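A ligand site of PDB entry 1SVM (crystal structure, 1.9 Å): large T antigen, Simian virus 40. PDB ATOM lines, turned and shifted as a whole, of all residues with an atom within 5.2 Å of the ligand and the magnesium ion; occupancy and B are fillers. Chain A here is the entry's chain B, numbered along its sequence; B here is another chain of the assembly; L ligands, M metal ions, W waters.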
ATOM      1  N   TRP A 143     -10.571   4.989   8.586  1.00  0.00           N
ATOM      2  CA  TRP A 143     -11.877   5.188   9.198  1.00  0.00           C
ATOM      3  C   TRP A 143     -12.967   4.826   8.194  1.00  0.00           C
ATOM      4  O   TRP A 143     -13.898   4.069   8.512  1.00  0.00           O
ATOM      5  CB  TRP A 143     -12.034   6.649   9.631  1.00  0.00           C
ATOM      6  CG  TRP A 143     -13.301   6.926  10.402  1.00  0.00           C
ATOM      7  CD1 TRP A 143     -13.452   6.962  11.760  1.00  0.00           C
ATOM      8  CD2 TRP A 143     -14.592   7.190   9.844  1.00  0.00           C
ATOM      9  NE1 TRP A 143     -14.762   7.225  12.080  1.00  0.00           N
ATOM     10  CE2 TRP A 143     -15.482   7.374  10.928  1.00  0.00           C
ATOM     11  CE3 TRP A 143     -15.090   7.293   8.532  1.00  0.00           C
ATOM     12  CZ2 TRP A 143     -16.844   7.649  10.735  1.00  0.00           C
ATOM     13  CZ3 TRP A 143     -16.435   7.567   8.341  1.00  0.00           C
ATOM     14  CH2 TRP A 143     -17.298   7.741   9.447  1.00  0.00           C
ATOM     15  N   LEU A 147     -16.434   1.960   7.820  1.00  0.00           N
ATOM     16  CA  LEU A 147     -17.818   2.433   7.755  1.00  0.00           C
ATOM     17  C   LEU A 147     -18.789   1.417   7.134  1.00  0.00           C
ATOM     18  O   LEU A 147     -19.964   1.349   7.521  1.00  0.00           O
ATOM     19  CB  LEU A 147     -17.895   3.753   6.974  1.00  0.00           C
ATOM     20  CG  LEU A 147     -19.270   4.395   6.786  1.00  0.00           C
ATOM     21  CD1 LEU A 147     -19.880   4.780   8.125  1.00  0.00           C
ATOM     22  CD2 LEU A 147     -19.124   5.603   5.875  1.00  0.00           C
ATOM     23  N   GLY A 176     -30.737   4.975   6.083  1.00  0.00           N
ATOM     24  CA  GLY A 176     -30.332   4.730   7.442  1.00  0.00           C
ATOM     25  C   GLY A 176     -30.690   5.860   8.400  1.00  0.00           C
ATOM     26  O   GLY A 176     -31.175   6.916   7.976  1.00  0.00           O
ATOM     27  N   PRO A 177     -30.446   5.661   9.701  1.00  0.00           N
ATOM     28  CA  PRO A 177     -30.733   6.644  10.752  1.00  0.00           C
ATOM     29  C   PRO A 177     -29.820   7.854  10.659  1.00  0.00           C
ATOM     30  O   PRO A 177     -28.858   7.871   9.874  1.00  0.00           O
ATOM     31  CB  PRO A 177     -30.456   5.860  12.047  1.00  0.00           C
ATOM     32  CG  PRO A 177     -30.480   4.420  11.635  1.00  0.00           C
ATOM     33  CD  PRO A 177     -29.861   4.445  10.276  1.00  0.00           C
ATOM     34  N   ILE A 178     -30.112   8.853  11.480  1.00  0.00           N
ATOM     35  CA  ILE A 178     -29.326  10.078  11.545  1.00  0.00           C
ATOM     36  C   ILE A 178     -27.890   9.760  11.968  1.00  0.00           C
ATOM     37  O   ILE A 178     -27.661   8.939  12.858  1.00  0.00           O
ATOM     38  CB  ILE A 178     -29.942  11.059  12.581  1.00  0.00           C
ATOM     39  CG1 ILE A 178     -31.320  11.496  12.102  1.00  0.00           C
ATOM     40  CG2 ILE A 178     -29.021  12.256  12.799  1.00  0.00           C
ATOM     41  CD1 ILE A 178     -32.087  12.319  13.117  1.00  0.00           C
ATOM     42  N   ASP A 179     -26.929  10.390  11.306  1.00  0.00           N
ATOM     43  CA  ASP A 179     -25.517  10.193  11.615  1.00  0.00           C
ATOM     44  C   ASP A 179     -25.039   8.752  11.462  1.00  0.00           C
ATOM     45  O   ASP A 179     -24.391   8.203  12.347  1.00  0.00           O
ATOM     46  CB  ASP A 179     -25.189  10.688  13.037  1.00  0.00           C
ATOM     47  CG  ASP A 179     -25.321  12.205  13.186  1.00  0.00           C
ATOM     48  OD1 ASP A 179     -25.395  12.907  12.150  1.00  0.00           O
ATOM     49  OD2 ASP A 179     -25.344  12.685  14.333  1.00  0.00           O
ATOM     50  N   SER A 180     -25.368   8.129  10.341  1.00  0.00           N
ATOM     51  CA  SER A 180     -24.928   6.763  10.082  1.00  0.00           C
ATOM     52  C   SER A 180     -23.875   6.765   8.969  1.00  0.00           C
ATOM     53  O   SER A 180     -23.342   5.718   8.615  1.00  0.00           O
ATOM     54  CB  SER A 180     -26.117   5.878   9.727  1.00  0.00           C
ATOM     55  OG  SER A 180     -26.862   6.425   8.649  1.00  0.00           O
ATOM     56  N   GLY A 181     -23.570   7.945   8.426  1.00  0.00           N
ATOM     57  CA  GLY A 181     -22.556   8.057   7.390  1.00  0.00           C
ATOM     58  C   GLY A 181     -22.997   8.203   5.947  1.00  0.00           C
ATOM     59  O   GLY A 181     -22.169   8.232   5.048  1.00  0.00           O
ATOM     60  N   LYS A 182     -24.304   8.327   5.714  1.00  0.00           N
ATOM     61  CA  LYS A 182     -24.849   8.452   4.365  1.00  0.00           C
ATOM     62  C   LYS A 182     -24.265   9.633   3.590  1.00  0.00           C
ATOM     63  O   LYS A 182     -23.731   9.492   2.484  1.00  0.00           O
ATOM     64  CB  LYS A 182     -26.364   8.601   4.420  1.00  0.00           C
ATOM     65  CG  LYS A 182     -27.089   7.458   5.115  1.00  0.00           C
ATOM     66  CD  LYS A 182     -28.604   7.644   5.076  1.00  0.00           C
ATOM     67  CE  LYS A 182     -29.040   8.898   5.819  1.00  0.00           C
ATOM     68  NZ  LYS A 182     -28.675   8.856   7.268  1.00  0.00           N
ATOM     69  N   THR A 183     -24.386  10.818   4.172  1.00  0.00           N
ATOM     70  CA  THR A 183     -23.897  12.045   3.564  1.00  0.00           C
ATOM     71  C   THR A 183     -22.382  12.025   3.449  1.00  0.00           C
ATOM     72  O   THR A 183     -21.837  12.472   2.441  1.00  0.00           O
ATOM     73  CB  THR A 183     -24.337  13.259   4.393  1.00  0.00           C
ATOM     74  OG1 THR A 183     -25.756  13.397   4.296  1.00  0.00           O
ATOM     75  CG2 THR A 183     -23.650  14.541   3.913  1.00  0.00           C
ATOM     76  N   THR A 184     -21.707  11.522   4.485  1.00  0.00           N
ATOM     77  CA  THR A 184     -20.250  11.473   4.474  1.00  0.00           C
ATOM     78  C   THR A 184     -19.744  10.712   3.240  1.00  0.00           C
ATOM     79  O   THR A 184     -18.866  11.197   2.523  1.00  0.00           O
ATOM     80  CB  THR A 184     -19.683  10.779   5.748  1.00  0.00           C
ATOM     81  OG1 THR A 184     -20.165  11.443   6.920  1.00  0.00           O
ATOM     82  CG2 THR A 184     -18.159  10.857   5.757  1.00  0.00           C
ATOM     83  N   GLU A 223     -29.686  14.627  -2.082  1.00  0.00           N
ATOM     84  CA  GLU A 223     -29.425  14.579  -0.653  1.00  0.00           C
ATOM     85  C   GLU A 223     -30.617  14.689   0.287  1.00  0.00           C
ATOM     86  O   GLU A 223     -31.507  15.524   0.099  1.00  0.00           O
ATOM     87  CB  GLU A 223     -28.402  15.653  -0.282  1.00  0.00           C
ATOM     88  CG  GLU A 223     -27.057  15.107   0.127  1.00  0.00           C
ATOM     89  CD  GLU A 223     -27.077  14.396   1.463  1.00  0.00           C
ATOM     90  OE1 GLU A 223     -27.248  15.072   2.491  1.00  0.00           O
ATOM     91  OE2 GLU A 223     -26.949  13.157   1.482  1.00  0.00           O
ATOM     92  N   ASP A 224     -30.595  13.855   1.319  1.00  0.00           N
ATOM     93  CA  ASP A 224     -31.612  13.827   2.357  1.00  0.00           C
ATOM     94  C   ASP A 224     -33.035  14.041   1.869  1.00  0.00           C
ATOM     95  O   ASP A 224     -33.680  15.040   2.208  1.00  0.00           O
ATOM     96  CB  ASP A 224     -31.265  14.870   3.425  1.00  0.00           C
ATOM     97  CG  ASP A 224     -31.475  14.351   4.826  1.00  0.00           C
ATOM     98  OD1 ASP A 224     -32.527  13.740   5.082  1.00  0.00           O
ATOM     99  OD2 ASP A 224     -30.585  14.576   5.677  1.00  0.00           O
ATOM    100  N   THR A 277     -29.996   9.734  -0.863  1.00  0.00           N
ATOM    101  CA  THR A 277     -29.763   9.425   0.559  1.00  0.00           C
ATOM    102  C   THR A 277     -31.052   9.787   1.309  1.00  0.00           C
ATOM    103  O   THR A 277     -31.694  10.786   0.972  1.00  0.00           O
ATOM    104  CB  THR A 277     -28.596  10.235   1.165  1.00  0.00           C
ATOM    105  OG1 THR A 277     -28.946  11.616   1.232  1.00  0.00           O
ATOM    106  CG2 THR A 277     -27.333  10.075   0.316  1.00  0.00           C
ATOM    107  N   ASN A 279     -33.643   9.018   5.268  1.00  0.00           N
ATOM    108  CA  ASN A 279     -33.900   8.534   6.627  1.00  0.00           C
ATOM    109  C   ASN A 279     -34.885   7.395   6.901  1.00  0.00           C
ATOM    110  O   ASN A 279     -35.709   7.513   7.818  1.00  0.00           O
ATOM    111  CB  ASN A 279     -34.371   9.684   7.505  1.00  0.00           C
ATOM    112  CG  ASN A 279     -33.249  10.509   8.051  1.00  0.00           C
ATOM    113  OD1 ASN A 279     -33.313  11.732   8.021  1.00  0.00           O
ATOM    114  ND2 ASN A 279     -32.221   9.856   8.562  1.00  0.00           N
ATOM    115  N   ARG A 298     -25.395   2.020   9.288  1.00  0.00           N
ATOM    116  CA  ARG A 298     -25.656   1.840  10.711  1.00  0.00           C
ATOM    117  C   ARG A 298     -24.686   2.612  11.593  1.00  0.00           C
ATOM    118  O   ARG A 298     -23.480   2.595  11.365  1.00  0.00           O
ATOM    119  CB  ARG A 298     -25.545   0.357  11.083  1.00  0.00           C
ATOM    120  CG  ARG A 298     -26.650  -0.547  10.573  1.00  0.00           C
ATOM    121  CD  ARG A 298     -26.459  -1.944  11.161  1.00  0.00           C
ATOM    122  NE  ARG A 298     -27.496  -2.891  10.765  1.00  0.00           N
ATOM    123  CZ  ARG A 298     -27.536  -4.151  11.168  1.00  0.00           C
ATOM    124  NH1 ARG A 298     -26.593  -4.626  11.984  1.00  0.00           N
ATOM    125  NH2 ARG A 298     -28.508  -4.956  10.766  1.00  0.00           N
ATOM    126  N   PRO A 299     -25.221   3.298  12.612  1.00  0.00           N
ATOM    127  CA  PRO A 299     -24.349   4.050  13.522  1.00  0.00           C
ATOM    128  C   PRO A 299     -23.456   3.024  14.230  1.00  0.00           C
ATOM    129  O   PRO A 299     -23.883   1.892  14.451  1.00  0.00           O
ATOM    130  CB  PRO A 299     -25.327   4.701  14.485  1.00  0.00           C
ATOM    131  CG  PRO A 299     -26.574   4.862  13.663  1.00  0.00           C
ATOM    132  CD  PRO A 299     -26.635   3.542  12.916  1.00  0.00           C
ATOM    133  N   LYS A 300     -22.233   3.413  14.556  1.00  0.00           N
ATOM    134  CA  LYS A 300     -21.304   2.521  15.253  1.00  0.00           C
ATOM    135  C   LYS A 300     -20.611   3.308  16.348  1.00  0.00           C
ATOM    136  O   LYS A 300     -19.991   4.334  16.075  1.00  0.00           O
ATOM    137  CB  LYS A 300     -20.269   1.946  14.284  1.00  0.00           C
ATOM    138  CG  LYS A 300     -20.860   1.096  13.179  1.00  0.00           C
ATOM    139  CD  LYS A 300     -19.770   0.497  12.291  1.00  0.00           C
ATOM    140  CE  LYS A 300     -20.352  -0.291  11.128  1.00  0.00           C
ATOM    141  NZ  LYS A 300     -19.289  -0.941  10.306  1.00  0.00           N
ATOM    142  N   ASP A 301     -20.726   2.840  17.581  1.00  0.00           N
ATOM    143  CA  ASP A 301     -20.108   3.550  18.694  1.00  0.00           C
ATOM    144  C   ASP A 301     -18.618   3.762  18.532  1.00  0.00           C
ATOM    145  O   ASP A 301     -18.117   4.847  18.833  1.00  0.00           O
ATOM    146  CB  ASP A 301     -20.372   2.823  20.016  1.00  0.00           C
ATOM    147  CG  ASP A 301     -20.453   1.321  19.860  1.00  0.00           C
ATOM    148  OD1 ASP A 301     -19.530   0.742  19.249  1.00  0.00           O
ATOM    149  OD2 ASP A 301     -21.441   0.734  20.347  1.00  0.00           O
ATOM    150  N   LEU A 303     -16.892   4.075  15.755  1.00  0.00           N
ATOM    151  CA  LEU A 303     -16.622   5.070  14.718  1.00  0.00           C
ATOM    152  C   LEU A 303     -16.758   6.441  15.366  1.00  0.00           C
ATOM    153  O   LEU A 303     -15.966   7.336  15.121  1.00  0.00           O
ATOM    154  CB  LEU A 303     -17.603   4.936  13.549  1.00  0.00           C
ATOM    155  CG  LEU A 303     -17.389   3.712  12.657  1.00  0.00           C
ATOM    156  CD1 LEU A 303     -18.459   3.680  11.551  1.00  0.00           C
ATOM    157  CD2 LEU A 303     -15.991   3.768  12.051  1.00  0.00           C
ATOM    158  N   LYS A 304     -17.778   6.569  16.220  1.00  0.00           N
ATOM    159  CA  LYS A 304     -18.049   7.803  16.941  1.00  0.00           C
ATOM    160  C   LYS A 304     -16.937   8.122  17.931  1.00  0.00           C
ATOM    161  O   LYS A 304     -16.418   9.234  17.949  1.00  0.00           O
ATOM    162  CB  LYS A 304     -19.389   7.672  17.675  1.00  0.00           C
ATOM    163  CG  LYS A 304     -19.775   8.869  18.536  1.00  0.00           C
ATOM    164  CD  LYS A 304     -21.173   8.693  19.138  1.00  0.00           C
ATOM    165  CE  LYS A 304     -21.610   9.913  19.939  1.00  0.00           C
ATOM    166  NZ  LYS A 304     -20.755  10.140  21.136  1.00  0.00           N
ATOM    167  N   LEU A 307     -13.665   9.255  16.211  1.00  0.00           N
ATOM    168  CA  LEU A 307     -13.708  10.648  15.763  1.00  0.00           C
ATOM    169  C   LEU A 307     -13.551  11.637  16.914  1.00  0.00           C
ATOM    170  O   LEU A 307     -12.952  12.706  16.750  1.00  0.00           O
ATOM    171  CB  LEU A 307     -15.021  10.923  15.023  1.00  0.00           C
ATOM    172  CG  LEU A 307     -15.164  10.266  13.652  1.00  0.00           C
ATOM    173  CD1 LEU A 307     -16.551  10.564  13.084  1.00  0.00           C
ATOM    174  CD2 LEU A 307     -14.082  10.798  12.714  1.00  0.00           C
ATOM    175  N   LEU A 314     -12.593  15.557  10.846  1.00  0.00           N
ATOM    176  CA  LEU A 314     -13.764  16.374  10.558  1.00  0.00           C
ATOM    177  C   LEU A 314     -13.363  17.825  10.279  1.00  0.00           C
ATOM    178  O   LEU A 314     -13.826  18.424   9.316  1.00  0.00           O
ATOM    179  CB  LEU A 314     -14.770  16.337  11.712  1.00  0.00           C
ATOM    180  CG  LEU A 314     -15.516  15.008  11.892  1.00  0.00           C
ATOM    181  CD1 LEU A 314     -16.434  15.083  13.095  1.00  0.00           C
ATOM    182  CD2 LEU A 314     -16.305  14.689  10.632  1.00  0.00           C
ATOM    183  N   ILE A 319     -12.713  12.652   5.959  1.00  0.00           N
ATOM    184  CA  ILE A 319     -13.536  11.468   5.689  1.00  0.00           C
ATOM    185  C   ILE A 319     -14.656  11.669   4.671  1.00  0.00           C
ATOM    186  O   ILE A 319     -15.228  10.696   4.189  1.00  0.00           O
ATOM    187  CB  ILE A 319     -14.123  10.855   6.984  1.00  0.00           C
ATOM    188  CG1 ILE A 319     -14.930  11.891   7.749  1.00  0.00           C
ATOM    189  CG2 ILE A 319     -12.986  10.299   7.848  1.00  0.00           C
ATOM    190  CD1 ILE A 319     -15.636  11.307   8.965  1.00  0.00           C
ATOM    191  N   GLN A 320     -14.944  12.917   4.338  1.00  0.00           N
ATOM    192  CA  GLN A 320     -15.976  13.210   3.350  1.00  0.00           C
ATOM    193  C   GLN A 320     -15.343  13.615   2.022  1.00  0.00           C
ATOM    194  O   GLN A 320     -16.031  14.081   1.101  1.00  0.00           O
ATOM    195  CB  GLN A 320     -16.904  14.335   3.852  1.00  0.00           C
ATOM    196  CG  GLN A 320     -16.209  15.472   4.622  1.00  0.00           C
ATOM    197  CD  GLN A 320     -16.053  15.207   6.138  1.00  0.00           C
ATOM    198  OE1 GLN A 320     -14.934  14.982   6.635  1.00  0.00           O
ATOM    199  NE2 GLN A 320     -17.188  15.239   6.872  1.00  0.00           N
ATOM    200  N   PRO B 167     -18.367  20.138   9.388  1.00  0.00           N
ATOM    201  CA  PRO B 167     -19.586  19.553   8.824  1.00  0.00           C
ATOM    202  C   PRO B 167     -20.536  19.111   9.935  1.00  0.00           C
ATOM    203  O   PRO B 167     -20.122  18.431  10.889  1.00  0.00           O
ATOM    204  CB  PRO B 167     -19.060  18.370   8.019  1.00  0.00           C
ATOM    205  CG  PRO B 167     -17.748  18.887   7.509  1.00  0.00           C
ATOM    206  CD  PRO B 167     -17.163  19.609   8.724  1.00  0.00           C
ATOM    207  N   LYS B 168     -21.801  19.513   9.817  1.00  0.00           N
ATOM    208  CA  LYS B 168     -22.853  19.169  10.770  1.00  0.00           C
ATOM    209  C   LYS B 168     -22.649  19.651  12.211  1.00  0.00           C
ATOM    210  O   LYS B 168     -23.364  19.213  13.116  1.00  0.00           O
ATOM    211  CB  LYS B 168     -23.098  17.661  10.741  1.00  0.00           C
ATOM    212  CG  LYS B 168     -24.569  17.286  10.936  1.00  0.00           C
ATOM    213  CD  LYS B 168     -24.833  15.823  10.580  1.00  0.00           C
ATOM    214  CE  LYS B 168     -26.317  15.515  10.584  1.00  0.00           C
ATOM    215  NZ  LYS B 168     -26.581  14.110  10.154  1.00  0.00           N
ATOM    216  N   LYS B 169     -21.689  20.546  12.427  1.00  0.00           N
ATOM    217  CA  LYS B 169     -21.429  21.119  13.749  1.00  0.00           C
ATOM    218  C   LYS B 169     -21.181  22.618  13.514  1.00  0.00           C
ATOM    219  O   LYS B 169     -20.283  23.213  14.103  1.00  0.00           O
ATOM    220  CB  LYS B 169     -20.185  20.486  14.376  1.00  0.00           C
ATOM    221  CG  LYS B 169     -20.366  19.024  14.763  1.00  0.00           C
ATOM    222  CD  LYS B 169     -19.107  18.498  15.473  1.00  0.00           C
ATOM    223  CE  LYS B 169     -19.329  17.123  16.078  1.00  0.00           C
ATOM    224  NZ  LYS B 169     -19.673  16.100  15.051  1.00  0.00           N
ATOM    225  N   ASP B 252     -25.918  21.310   7.080  1.00  0.00           N
ATOM    226  CA  ASP B 252     -24.807  20.369   7.270  1.00  0.00           C
ATOM    227  C   ASP B 252     -23.487  20.919   6.747  1.00  0.00           C
ATOM    228  O   ASP B 252     -22.442  20.757   7.380  1.00  0.00           O
ATOM    229  CB  ASP B 252     -25.076  19.035   6.571  1.00  0.00           C
ATOM    230  CG  ASP B 252     -26.156  18.226   7.247  1.00  0.00           C
ATOM    231  OD1 ASP B 252     -26.403  18.476   8.436  1.00  0.00           O
ATOM    232  OD2 ASP B 252     -26.729  17.337   6.587  1.00  0.00           O
ATOM    233  N   SER B 254     -21.773  19.798   4.260  1.00  0.00           N
ATOM    234  CA  SER B 254     -20.891  18.716   3.834  1.00  0.00           C
ATOM    235  C   SER B 254     -20.792  18.740   2.323  1.00  0.00           C
ATOM    236  O   SER B 254     -19.706  18.639   1.759  1.00  0.00           O
ATOM    237  CB  SER B 254     -21.409  17.347   4.271  1.00  0.00           C
ATOM    238  OG  SER B 254     -21.190  17.169   5.653  1.00  0.00           O
ATOM    239  N   ALA B 289     -30.366  17.767  15.167  1.00  0.00           N
ATOM    240  CA  ALA B 289     -29.069  17.145  14.928  1.00  0.00           C
ATOM    241  C   ALA B 289     -28.119  18.074  14.155  1.00  0.00           C
ATOM    242  O   ALA B 289     -26.916  17.802  14.083  1.00  0.00           O
ATOM    243  CB  ALA B 289     -29.251  15.830  14.170  1.00  0.00           C
ATOM    244  N   ARG B 290     -28.652  19.144  13.576  1.00  0.00           N
ATOM    245  CA  ARG B 290     -27.826  20.084  12.827  1.00  0.00           C
ATOM    246  C   ARG B 290     -27.321  21.204  13.754  1.00  0.00           C
ATOM    247  O   ARG B 290     -26.446  21.981  13.369  1.00  0.00           O
ATOM    248  CB  ARG B 290     -28.610  20.702  11.659  1.00  0.00           C
ATOM    249  CG  ARG B 290     -29.324  19.726  10.689  1.00  0.00           C
ATOM    250  CD  ARG B 290     -28.678  18.361  10.628  1.00  0.00           C
ATOM    251  NE  ARG B 290     -28.681  17.770   9.287  1.00  0.00           N
ATOM    252  CZ  ARG B 290     -29.374  16.697   8.931  1.00  0.00           C
ATOM    253  NH1 ARG B 290     -30.151  16.076   9.804  1.00  0.00           N
ATOM    254  NH2 ARG B 290     -29.239  16.207   7.707  1.00  0.00           N
HETATM  255  P1  LIG L   1     -28.525  12.434   8.441  1.00  0.00           P
HETATM  256  O1  LIG L   1     -28.253  13.207   7.174  1.00  0.00           O
HETATM  257  O2  LIG L   1     -28.856  13.340   9.660  1.00  0.00           O
HETATM  258  O3  LIG L   1     -29.724  11.497   8.153  1.00  0.00           O
HETATM  259  P2  LIG L   1     -26.330  10.690   7.706  1.00  0.00           P
HETATM  260  O4  LIG L   1     -25.550   9.614   8.303  1.00  0.00           O
HETATM  261  O5  LIG L   1     -25.926  11.475   6.463  1.00  0.00           O
HETATM  262  O6  LIG L   1     -27.324  11.352   8.771  1.00  0.00           O
HETATM  263  P3  LIG L   1     -23.828  12.246   7.847  1.00  0.00           P
HETATM  264  O7  LIG L   1     -23.809  13.679   8.191  1.00  0.00           O
HETATM  265  O8  LIG L   1     -22.693  11.396   7.324  1.00  0.00           O
HETATM  266  O9  LIG L   1     -25.034  11.346   8.468  1.00  0.00           O
HETATM  267  O10 LIG L   1     -23.186  12.084   9.315  1.00  0.00           O
HETATM  268  C1  LIG L   1     -21.834  12.482   9.512  1.00  0.00           C
HETATM  269  C2  LIG L   1     -21.432  12.657  10.975  1.00  0.00           C
HETATM  270  O11 LIG L   1     -22.004  11.679  11.831  1.00  0.00           O
HETATM  271  C3  LIG L   1     -19.947  12.519  11.043  1.00  0.00           C
HETATM  272  O12 LIG L   1     -19.405  13.817  10.972  1.00  0.00           O
HETATM  273  C4  LIG L   1     -19.700  11.750  12.352  1.00  0.00           C
HETATM  274  O13 LIG L   1     -19.420  12.495  13.495  1.00  0.00           O
HETATM  275  C5  LIG L   1     -20.960  10.918  12.495  1.00  0.00           C
HETATM  276  N1  LIG L   1     -21.088   9.536  11.866  1.00  0.00           N
HETATM  277  C6  LIG L   1     -21.198   9.262  10.516  1.00  0.00           C
HETATM  278  N2  LIG L   1     -21.300   7.964  10.365  1.00  0.00           N
HETATM  279  C7  LIG L   1     -21.268   7.322  11.555  1.00  0.00           C
HETATM  280  C8  LIG L   1     -21.344   5.996  11.998  1.00  0.00           C
HETATM  281  N3  LIG L   1     -21.537   4.927  11.240  1.00  0.00           N
HETATM  282  N4  LIG L   1     -21.260   5.727  13.368  1.00  0.00           N
HETATM  283  C9  LIG L   1     -21.120   6.748  14.292  1.00  0.00           C
HETATM  284  N5  LIG L   1     -21.054   8.063  13.882  1.00  0.00           N
HETATM  285  C10 LIG L   1     -21.128   8.337  12.529  1.00  0.00           C
HETATM  286 MG    MG M   1     -27.090  13.292   5.742  1.00  0.00          MG
HETATM  287  O   HOH W   1     -28.330  12.135   4.312  1.00  0.00           O
HETATM  288  O   HOH W   2     -25.930  14.465   7.108  1.00  0.00           O
HETATM  289  O   HOH W   3     -31.777  13.701   8.893  1.00  0.00           O
HETATM  290  O   HOH W   4     -28.021  15.131   5.029  1.00  0.00           O
HETATM  291  O   HOH W   5     -21.803  15.530   7.388  1.00  0.00           O
HETATM  292  O   HOH W   6     -31.042  11.498   5.530  1.00  0.00           O
HETATM  293  O   HOH W   7     -19.979  16.060  12.217  1.00  0.00           O
HETATM  294  O   HOH W   8     -24.280   8.037  15.116  1.00  0.00           O
HETATM  295  O   HOH W   9     -19.513  13.892   8.082  1.00  0.00           O
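Water W2 lies within hydrogen-bond range of O7 of the ligand (2.5 Å), OD2 of Asp 252 of chain B (3.0 Å) and NZ of Lys 168 of chain B (3.1 Å).
Water W7 lies within hydrogen-bond range of O12 of the ligand (2.6 Å), O of Pro 167 of chain B (2.7 Å) and NZ of Lys 169 of chain B (2.9 Å).
Water W5 lies within hydrogen-bond range of OG of Ser 254 of chain B (2.5 Å) and O7 of the ligand (2.8 Å).
Water W6 lies within hydrogen-bond range of the side-chain carboxylate (OD1) of Asp 224, an oxygen (O3) of the ligand and the side-chain amide oxygen (OD1) of Asn 279.
Water W3 lies within hydrogen-bond range of the side-chain amide oxygen (OD1) of Asn 279, the guanidinium group (NH1) of Arg 290 of chain B and an oxygen (O2) of the ligand.
Water W8 bridges the backbone carbonyl oxygen of Asp 179 (2.8 Å) and a nitrogen (N5) of the ligand (3.5 Å).
The magnesium ion is bound by O1 of the ligand, OG1 of Thr 183, water W2, water W4, water W1 and O5 of the ligand.
The magnesium ion has six donor atoms within binding distance.
The backbone NH of Thr 183 sits close to an oxygen (O5) of the ligand (2.8 Å).
The side-chain amino group of Lys 168 of chain B lies within salt-bridge range of an oxygen (O2) of the ligand (2.5 Å).
N of Ser 180 lies within hydrogen-bond range of O4 of the ligand.
The backbone carbonyl oxygen (O) of Ser 180 sits at hydrogen-bond distance from a nitrogen (N3) of the ligand, 3.3 Å away.
OG of Ser 180 sits close to O4 of the ligand, 3.5 Å away.
O8 of the ligand is in hydrogen-bond range of N of Thr 184 (3.0 Å).
An oxygen (O8) of the ligand lies within hydrogen-bond range of the side-chain hydroxyl of Thr 184 (2.6 Å).
N of Gly 181 lies within hydrogen-bond range of O4 of the ligand (2.6 Å).
The backbone NH (N) of Asp 179 is in hydrogen-bond range of an oxygen (O6) of the ligand (2.7 Å).
N of Lys 300 is in hydrogen-bond range of N4 of the ligand (2.8 Å).
O4 of the ligand is in hydrogen-bond range of N of Lys 182 (3.1 Å).
An oxygen (O3) of the ligand lies within salt-bridge range of the side-chain amino group (NZ) of Lys 182 (3.0 Å).
An oxygen (O3) of the ligand is in hydrogen-bond range of the side-chain amide nitrogen (ND2) of Asn 279 (3.0 Å).
The guanidinium group of Arg 290 of chain B lies within salt-bridge range of an oxygen (O2) of the ligand.
The backbone carbonyl oxygen (O) of Arg 298 is in hydrogen-bond range of a nitrogen (N3) of the ligand.
The side-chain hydroxyl (OG1) of Thr 183 sits close to the side-chain carboxylate (OE1) of Glu 223 (2.9 Å).
OG of Ser 180 lies within hydrogen-bond range of NZ of Lys 182, at 3.3 Å.
The side-chain hydroxyl (OG) of Ser 180 sits at hydrogen-bond distance from the backbone carbonyl oxygen (O) of Pro 177, 2.8 Å away.
The side-chain amino group (NZ) of Lys 182 lies within hydrogen-bond range of the backbone carbonyl oxygen (O) of Gly 176 (3.2 Å).
The backbone carbonyl oxygen (O) of Gly 176 is in hydrogen-bond range of the side-chain amide nitrogen (ND2) of Asn 279, 3.2 Å away.
The side-chain carboxylate (OD2) of Asp 224 is in salt-bridge range of the guanidinium group (NH2) of Arg 290 of chain B.
The side-chain carboxylate (OD1) of Asp 252 of chain B lies within salt-bridge range of the guanidinium group (NE) of Arg 290 of chain B.
The side-chain hydroxyl (OG1) of Thr 277 is in hydrogen-bond range of the side-chain carboxylate (OE2) of Glu 223 (2.5 Å).
OE1 of Glu 223 touches the magnesium ion (3.7 Å).
Asp 224 touches the magnesium ion (OD2 to MG, 3.7 Å).
Of the 32 residues printed, 3 come within 4 Å of the magnesium ion.
The nearest printed residue that does not touch the magnesium ion is Arg 290 of chain B (4.1 Å).
O1 of the ligand sits close to OD2 of Asp 224 (3.1 Å).
Merely in contact with the ligand: Leu 147 (3.5 Å), Pro 177 (3.96 Å), Ile 178 (3.3 Å), Pro 299 (3.5 Å), Leu 303 (3.3 Å), Lys 304 (3.9 Å), Leu 307 (3.4 Å), Leu 314 (3.2 Å) and Lys 169 of chain B (3.9 Å).
Hydrophobic or aromatic side chains that line the ligand: Leu 147, Ile 178, Leu 303, Leu 307 and Leu 314.
Of the 32 residues printed, 21 come within 4 Å of the ligand.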
